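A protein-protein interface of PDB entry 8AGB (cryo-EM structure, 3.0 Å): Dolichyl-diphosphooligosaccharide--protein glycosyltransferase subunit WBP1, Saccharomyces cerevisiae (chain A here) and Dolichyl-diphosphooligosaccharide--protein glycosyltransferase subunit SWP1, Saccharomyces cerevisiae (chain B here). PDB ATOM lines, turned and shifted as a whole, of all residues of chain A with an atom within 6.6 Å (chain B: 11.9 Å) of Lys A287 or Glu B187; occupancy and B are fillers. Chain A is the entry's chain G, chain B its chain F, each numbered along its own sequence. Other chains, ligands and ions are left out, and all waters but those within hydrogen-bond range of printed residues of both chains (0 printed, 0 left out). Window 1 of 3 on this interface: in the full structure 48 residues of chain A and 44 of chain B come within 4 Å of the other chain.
The side-chain carboxylate (OE2) of Glu B187 is in salt-bridge range of the side-chain amino group (NZ) of Lys A287, 3.7 Å away. NE2 of His B182 lies within hydrogen-bond range of OD1 of Asp A348 (2.8 Å).
N of Lys A287 sits at hydrogen-bond distance from O of Pro A347, at 3.3 Å. The backbone carbonyl oxygen of Leu A346 is in hydrogen-bond range of the backbone NH of Lys A287. O of Asp A288 sits close to N of Leu A346, at 3.4 Å.
Among the printed residues, pairs that only touch across the chains: Ile A345 with Phe B184, Leu A346 with Phe B184, Pro A347 with His B182, Pro A347 with Phe B184, Asp A348 with Phe B184 and Asp A348 with His B185.
Of the printed residues of chain B, Lys A287 touches Glu B187. Glu B187 touches just one residue of chain A: Lys A287 (3.7 Å). Printed residues of chain B within 4 Å of Leu A346: Phe B184. Asp A348 touches just these residues of chain B: His B182, Phe B184 and His B185. Printed residues of chain A within 4 Å of Phe B184: Ile A345 (3.5 Å), Leu A346 (3.2 Å), Pro A347 (3.7 Å) and Asp A348 (3.2 Å). Of the printed residues of chain A, His B182 touches Pro A347 and Asp A348. Printed residues of chain A within 4 Å of His B185: Asp A348. Leu A378 touches none of the printed residues of chain B. The nearest residue of chain B that does not touch Lys A287 is Phe B184 (4.1 Å). The nearest printed residue of chain A that does not touch Glu B187 is Leu A378 (7.2 Å). The nearest printed residue of chain A that does not touch Phe B184 is Lys A287 (4.1 Å).
Of the 12 printed residues of chain A, 5 touch a printed residue of chain B. Printed residues of chain A that touch a printed residue of chain B: Lys A287, Ile A345, Leu A346, Pro A347 and Asp A348. Hydrophobic or aromatic side chains of chain A within 4 Å of the printed part of chain B: Pro A347. Of the 10 printed residues of chain B, 4 touch a printed residue of chain A. Printed residues of chain B that touch a printed residue of chain A: His B182, Phe B184, His B185 and Glu B187. Among the printed residues, Asp or Glu carboxylates within 4 Å of a Lys or Arg side-chain nitrogen of the other chain: Lys A287 with Glu B187 (3.7 Å).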
ATOM      1  N   LYS A 285     -10.737 -28.968  20.563  1.00  0.00           N
ATOM      2  CA  LYS A 285     -11.616 -27.866  20.205  1.00  0.00           C
ATOM      3  C   LYS A 285     -10.825 -26.894  19.343  1.00  0.00           C
ATOM      4  O   LYS A 285      -9.630 -27.080  19.101  1.00  0.00           O
ATOM      5  CB  LYS A 285     -12.180 -27.181  21.452  1.00  0.00           C
ATOM      6  CG  LYS A 285     -11.111 -26.617  22.357  1.00  0.00           C
ATOM      7  CD  LYS A 285     -11.699 -25.882  23.540  1.00  0.00           C
ATOM      8  CE  LYS A 285     -10.642 -25.028  24.214  1.00  0.00           C
ATOM      9  NZ  LYS A 285     -10.997 -24.700  25.618  1.00  0.00           N
ATOM     10  N   ILE A 286     -11.496 -25.843  18.873  1.00  0.00           N
ATOM     11  CA  ILE A 286     -10.840 -24.883  17.997  1.00  0.00           C
ATOM     12  C   ILE A 286      -9.834 -24.062  18.792  1.00  0.00           C
ATOM     13  O   ILE A 286     -10.075 -23.697  19.951  1.00  0.00           O
ATOM     14  CB  ILE A 286     -11.880 -23.989  17.298  1.00  0.00           C
ATOM     15  CG1 ILE A 286     -12.591 -23.087  18.306  1.00  0.00           C
ATOM     16  CG2 ILE A 286     -12.879 -24.835  16.533  1.00  0.00           C
ATOM     17  CD1 ILE A 286     -13.835 -22.429  17.762  1.00  0.00           C
ATOM     18  N   LYS A 287      -8.678 -23.802  18.180  1.00  0.00           N
ATOM     19  CA  LYS A 287      -7.605 -23.015  18.787  1.00  0.00           C
ATOM     20  C   LYS A 287      -7.113 -23.672  20.077  1.00  0.00           C
ATOM     21  O   LYS A 287      -7.119 -23.079  21.157  1.00  0.00           O
ATOM     22  CB  LYS A 287      -8.053 -21.570  19.029  1.00  0.00           C
ATOM     23  CG  LYS A 287      -8.543 -20.856  17.784  1.00  0.00           C
ATOM     24  CD  LYS A 287      -9.108 -19.484  18.111  1.00  0.00           C
ATOM     25  CE  LYS A 287      -9.972 -19.523  19.358  1.00  0.00           C
ATOM     26  NZ  LYS A 287     -10.439 -18.171  19.755  1.00  0.00           N
ATOM     27  N   ASP A 288      -6.681 -24.922  19.940  1.00  0.00           N
ATOM     28  CA  ASP A 288      -6.162 -25.716  21.047  1.00  0.00           C
ATOM     29  C   ASP A 288      -4.796 -26.243  20.648  1.00  0.00           C
ATOM     30  O   ASP A 288      -4.671 -26.916  19.622  1.00  0.00           O
ATOM     31  CB  ASP A 288      -7.109 -26.871  21.379  1.00  0.00           C
ATOM     32  CG  ASP A 288      -7.079 -27.248  22.841  1.00  0.00           C
ATOM     33  OD1 ASP A 288      -6.094 -26.906  23.527  1.00  0.00           O
ATOM     34  OD2 ASP A 288      -8.044 -27.890  23.305  1.00  0.00           O
ATOM     35  N   LYS A 289      -3.775 -25.942  21.447  1.00  0.00           N
ATOM     36  CA  LYS A 289      -2.419 -26.320  21.073  1.00  0.00           C
ATOM     37  C   LYS A 289      -2.281 -27.835  21.061  1.00  0.00           C
ATOM     38  O   LYS A 289      -2.675 -28.515  22.012  1.00  0.00           O
ATOM     39  CB  LYS A 289      -1.405 -25.705  22.031  1.00  0.00           C
ATOM     40  CG  LYS A 289      -1.125 -24.242  21.762  1.00  0.00           C
ATOM     41  CD  LYS A 289       0.360 -23.951  21.824  1.00  0.00           C
ATOM     42  CE  LYS A 289       0.664 -22.563  21.291  1.00  0.00           C
ATOM     43  NZ  LYS A 289       2.067 -22.450  20.811  1.00  0.00           N
ATOM     44  N   ILE A 345      -1.238 -24.605  16.603  1.00  0.00           N
ATOM     45  CA  ILE A 345      -2.567 -24.302  17.117  1.00  0.00           C
ATOM     46  C   ILE A 345      -3.586 -24.750  16.082  1.00  0.00           C
ATOM     47  O   ILE A 345      -3.523 -24.329  14.921  1.00  0.00           O
ATOM     48  CB  ILE A 345      -2.721 -22.805  17.423  1.00  0.00           C
ATOM     49  CG1 ILE A 345      -1.548 -22.307  18.261  1.00  0.00           C
ATOM     50  CG2 ILE A 345      -4.031 -22.542  18.139  1.00  0.00           C
ATOM     51  CD1 ILE A 345      -1.675 -20.863  18.676  1.00  0.00           C
ATOM     52  N   LEU A 346      -4.517 -25.611  16.494  1.00  0.00           N
ATOM     53  CA  LEU A 346      -5.578 -26.071  15.607  1.00  0.00           C
ATOM     54  C   LEU A 346      -6.327 -24.881  15.018  1.00  0.00           C
ATOM     55  O   LEU A 346      -6.323 -23.795  15.610  1.00  0.00           O
ATOM     56  CB  LEU A 346      -6.544 -26.986  16.361  1.00  0.00           C
ATOM     57  CG  LEU A 346      -5.965 -28.263  16.958  1.00  0.00           C
ATOM     58  CD1 LEU A 346      -7.008 -28.954  17.805  1.00  0.00           C
ATOM     59  CD2 LEU A 346      -5.483 -29.177  15.855  1.00  0.00           C
ATOM     60  N   PRO A 347      -6.993 -25.040  13.876  1.00  0.00           N
ATOM     61  CA  PRO A 347      -7.665 -23.892  13.263  1.00  0.00           C
ATOM     62  C   PRO A 347      -8.910 -23.481  14.027  1.00  0.00           C
ATOM     63  O   PRO A 347      -9.294 -24.138  14.998  1.00  0.00           O
ATOM     64  CB  PRO A 347      -7.994 -24.411  11.861  1.00  0.00           C
ATOM     65  CG  PRO A 347      -8.292 -25.836  12.114  1.00  0.00           C
ATOM     66  CD  PRO A 347      -7.188 -26.253  13.062  1.00  0.00           C
ATOM     67  N   ASP A 348      -9.551 -22.399  13.597  1.00  0.00           N
ATOM     68  CA  ASP A 348     -10.736 -21.884  14.261  1.00  0.00           C
ATOM     69  C   ASP A 348     -12.013 -22.370  13.599  1.00  0.00           C
ATOM     70  O   ASP A 348     -13.096 -21.867  13.908  1.00  0.00           O
ATOM     71  CB  ASP A 348     -10.705 -20.356  14.290  1.00  0.00           C
ATOM     72  CG  ASP A 348      -9.959 -19.770  13.113  1.00  0.00           C
ATOM     73  OD1 ASP A 348     -10.000 -20.371  12.019  1.00  0.00           O
ATOM     74  OD2 ASP A 348      -9.330 -18.706  13.279  1.00  0.00           O
ATOM     75  N   ARG A 349     -11.904 -23.336  12.694  1.00  0.00           N
ATOM     76  CA  ARG A 349     -13.040 -23.948  12.023  1.00  0.00           C
ATOM     77  C   ARG A 349     -13.235 -25.339  12.611  1.00  0.00           C
ATOM     78  O   ARG A 349     -12.304 -26.150  12.610  1.00  0.00           O
ATOM     79  CB  ARG A 349     -12.787 -24.011  10.517  1.00  0.00           C
ATOM     80  CG  ARG A 349     -13.590 -25.041   9.761  1.00  0.00           C
ATOM     81  CD  ARG A 349     -14.923 -24.485   9.310  1.00  0.00           C
ATOM     82  NE  ARG A 349     -15.416 -25.186   8.130  1.00  0.00           N
ATOM     83  CZ  ARG A 349     -15.497 -24.642   6.922  1.00  0.00           C
ATOM     84  NH1 ARG A 349     -15.950 -25.354   5.901  1.00  0.00           N
ATOM     85  NH2 ARG A 349     -15.121 -23.386   6.734  1.00  0.00           N
ATOM     86  N   ILE A 375     -12.738 -31.909  15.651  1.00  0.00           N
ATOM     87  CA  ILE A 375     -12.426 -30.675  16.361  1.00  0.00           C
ATOM     88  C   ILE A 375     -13.747 -29.982  16.669  1.00  0.00           C
ATOM     89  O   ILE A 375     -14.461 -29.544  15.762  1.00  0.00           O
ATOM     90  CB  ILE A 375     -11.492 -29.777  15.544  1.00  0.00           C
ATOM     91  CG1 ILE A 375     -10.493 -30.630  14.765  1.00  0.00           C
ATOM     92  CG2 ILE A 375     -10.765 -28.811  16.447  1.00  0.00           C
ATOM     93  CD1 ILE A 375      -9.394 -31.211  15.612  1.00  0.00           C
ATOM     94  N   LEU A 378     -16.289 -24.155  20.758  1.00  0.00           N
ATOM     95  CA  LEU A 378     -16.227 -23.680  22.133  1.00  0.00           C
ATOM     96  C   LEU A 378     -17.566 -23.885  22.829  1.00  0.00           C
ATOM     97  O   LEU A 378     -18.612 -23.457  22.334  1.00  0.00           O
ATOM     98  CB  LEU A 378     -15.836 -22.205  22.166  1.00  0.00           C
ATOM     99  CG  LEU A 378     -14.369 -21.884  21.895  1.00  0.00           C
ATOM    100  CD1 LEU A 378     -14.095 -20.419  22.166  1.00  0.00           C
ATOM    101  CD2 LEU A 378     -13.471 -22.760  22.744  1.00  0.00           C
ATOM    102  N   HIS B 182      -2.388 -21.881   9.027  1.00  0.00           N
ATOM    103  CA  HIS B 182      -3.691 -21.238   9.091  1.00  0.00           C
ATOM    104  C   HIS B 182      -3.527 -19.789   9.532  1.00  0.00           C
ATOM    105  O   HIS B 182      -2.576 -19.435  10.235  1.00  0.00           O
ATOM    106  CB  HIS B 182      -4.614 -21.988  10.051  1.00  0.00           C
ATOM    107  CG  HIS B 182      -6.057 -21.613   9.925  1.00  0.00           C
ATOM    108  ND1 HIS B 182      -6.898 -22.193   9.000  1.00  0.00           N
ATOM    109  CD2 HIS B 182      -6.811 -20.722  10.611  1.00  0.00           C
ATOM    110  CE1 HIS B 182      -8.107 -21.673   9.119  1.00  0.00           C
ATOM    111  NE2 HIS B 182      -8.080 -20.778  10.090  1.00  0.00           N
ATOM    112  N   ILE B 183      -4.457 -18.943   9.107  1.00  0.00           N
ATOM    113  CA  ILE B 183      -4.453 -17.528   9.457  1.00  0.00           C
ATOM    114  C   ILE B 183      -5.653 -17.260  10.350  1.00  0.00           C
ATOM    115  O   ILE B 183      -6.805 -17.343   9.905  1.00  0.00           O
ATOM    116  CB  ILE B 183      -4.480 -16.627   8.216  1.00  0.00           C
ATOM    117  CG1 ILE B 183      -3.426 -17.076   7.209  1.00  0.00           C
ATOM    118  CG2 ILE B 183      -4.251 -15.179   8.607  1.00  0.00           C
ATOM    119  CD1 ILE B 183      -3.332 -16.181   6.003  1.00  0.00           C
ATOM    120  N   PHE B 184      -5.385 -16.931  11.606  1.00  0.00           N
ATOM    121  CA  PHE B 184      -6.431 -16.662  12.577  1.00  0.00           C
ATOM    122  C   PHE B 184      -6.771 -15.179  12.561  1.00  0.00           C
ATOM    123  O   PHE B 184      -5.950 -14.340  12.185  1.00  0.00           O
ATOM    124  CB  PHE B 184      -5.996 -17.087  13.979  1.00  0.00           C
ATOM    125  CG  PHE B 184      -5.569 -18.522  14.073  1.00  0.00           C
ATOM    126  CD1 PHE B 184      -4.270 -18.892  13.781  1.00  0.00           C
ATOM    127  CD2 PHE B 184      -6.466 -19.501  14.454  1.00  0.00           C
ATOM    128  CE1 PHE B 184      -3.877 -20.208  13.863  1.00  0.00           C
ATOM    129  CE2 PHE B 184      -6.077 -20.817  14.538  1.00  0.00           C
ATOM    130  CZ  PHE B 184      -4.782 -21.171  14.243  1.00  0.00           C
ATOM    131  N   HIS B 185      -7.992 -14.863  12.968  1.00  0.00           N
ATOM    132  CA  HIS B 185      -8.412 -13.475  13.036  1.00  0.00           C
ATOM    133  C   HIS B 185      -7.983 -12.863  14.362  1.00  0.00           C
ATOM    134  O   HIS B 185      -7.732 -13.562  15.346  1.00  0.00           O
ATOM    135  CB  HIS B 185      -9.927 -13.355  12.873  1.00  0.00           C
ATOM    136  CG  HIS B 185     -10.532 -14.440  12.040  1.00  0.00           C
ATOM    137  ND1 HIS B 185     -11.502 -15.292  12.522  1.00  0.00           N
ATOM    138  CD2 HIS B 185     -10.305 -14.814  10.759  1.00  0.00           C
ATOM    139  CE1 HIS B 185     -11.846 -16.145  11.573  1.00  0.00           C
ATOM    140  NE2 HIS B 185     -11.134 -15.876  10.493  1.00  0.00           N
ATOM    141  N   ALA B 186      -7.902 -11.537  14.377  1.00  0.00           N
ATOM    142  CA  ALA B 186      -7.556 -10.817  15.593  1.00  0.00           C
ATOM    143  C   ALA B 186      -8.793 -10.719  16.472  1.00  0.00           C
ATOM    144  O   ALA B 186      -9.831 -10.207  16.036  1.00  0.00           O
ATOM    145  CB  ALA B 186      -7.012  -9.430  15.262  1.00  0.00           C
ATOM    146  N   GLU B 187      -8.688 -11.221  17.698  1.00  0.00           N
ATOM    147  CA  GLU B 187      -9.822 -11.196  18.604  1.00  0.00           C
ATOM    148  C   GLU B 187     -10.229  -9.752  18.894  1.00  0.00           C
ATOM    149  O   GLU B 187      -9.397  -8.842  18.832  1.00  0.00           O
ATOM    150  CB  GLU B 187      -9.471 -11.922  19.902  1.00  0.00           C
ATOM    151  CG  GLU B 187      -8.626 -13.168  19.699  1.00  0.00           C
ATOM    152  CD  GLU B 187      -9.152 -14.363  20.470  1.00  0.00           C
ATOM    153  OE1 GLU B 187     -10.363 -14.387  20.778  1.00  0.00           O
ATOM    154  OE2 GLU B 187      -8.356 -15.278  20.765  1.00  0.00           O
ATOM    155  N   PRO B 188     -11.505  -9.512  19.197  1.00  0.00           N
ATOM    156  CA  PRO B 188     -11.968  -8.132  19.385  1.00  0.00           C
ATOM    157  C   PRO B 188     -11.229  -7.446  20.522  1.00  0.00           C
ATOM    158  O   PRO B 188     -10.894  -8.065  21.534  1.00  0.00           O
ATOM    159  CB  PRO B 188     -13.460  -8.297  19.685  1.00  0.00           C
ATOM    160  CG  PRO B 188     -13.585  -9.677  20.204  1.00  0.00           C
ATOM    161  CD  PRO B 188     -12.567 -10.491  19.480  1.00  0.00           C
ATOM    162  N   LYS B 189     -10.979  -6.154  20.347  1.00  0.00           N
ATOM    163  CA  LYS B 189     -10.205  -5.399  21.319  1.00  0.00           C
ATOM    164  C   LYS B 189     -11.074  -4.978  22.497  1.00  0.00           C
ATOM    165  O   LYS B 189     -12.281  -4.760  22.364  1.00  0.00           O
ATOM    166  CB  LYS B 189      -9.580  -4.168  20.665  1.00  0.00           C
ATOM    167  CG  LYS B 189      -8.456  -3.535  21.472  1.00  0.00           C
ATOM    168  CD  LYS B 189      -8.719  -2.058  21.716  1.00  0.00           C
ATOM    169  CE  LYS B 189      -7.669  -1.455  22.634  1.00  0.00           C
ATOM    170  NZ  LYS B 189      -7.892   0.002  22.844  1.00  0.00           N
ATOM    171  N   ARG B 190     -10.438  -4.862  23.658  1.00  0.00           N
ATOM    172  CA  ARG B 190     -11.096  -4.488  24.902  1.00  0.00           C
ATOM    173  C   ARG B 190     -10.590  -3.119  25.328  1.00  0.00           C
ATOM    174  O   ARG B 190      -9.382  -2.866  25.296  1.00  0.00           O
ATOM    175  CB  ARG B 190     -10.830  -5.523  25.994  1.00  0.00           C
ATOM    176  CG  ARG B 190     -11.118  -6.949  25.568  1.00  0.00           C
ATOM    177  CD  ARG B 190     -10.447  -7.946  26.492  1.00  0.00           C
ATOM    178  NE  ARG B 190     -10.802  -9.322  26.160  1.00  0.00           N
ATOM    179  CZ  ARG B 190     -10.525 -10.368  26.929  1.00  0.00           C
ATOM    180  NH1 ARG B 190      -9.887 -10.197  28.078  1.00  0.00           N
ATOM    181  NH2 ARG B 190     -10.885 -11.586  26.551  1.00  0.00           N
ATOM    182  N   VAL B 191     -11.518  -2.239  25.708  1.00  0.00           N
ATOM    183  CA  VAL B 191     -11.208  -0.861  26.079  1.00  0.00           C
ATOM    184  C   VAL B 191     -10.109  -0.841  27.133  1.00  0.00           C
ATOM    185  O   VAL B 191     -10.025  -1.742  27.974  1.00  0.00           O
ATOM    186  CB  VAL B 191     -12.470  -0.136  26.584  1.00  0.00           C
ATOM    187  CG1 VAL B 191     -13.085  -0.885  27.753  1.00  0.00           C
ATOM    188  CG2 VAL B 191     -12.166   1.307  26.957  1.00  0.00           C
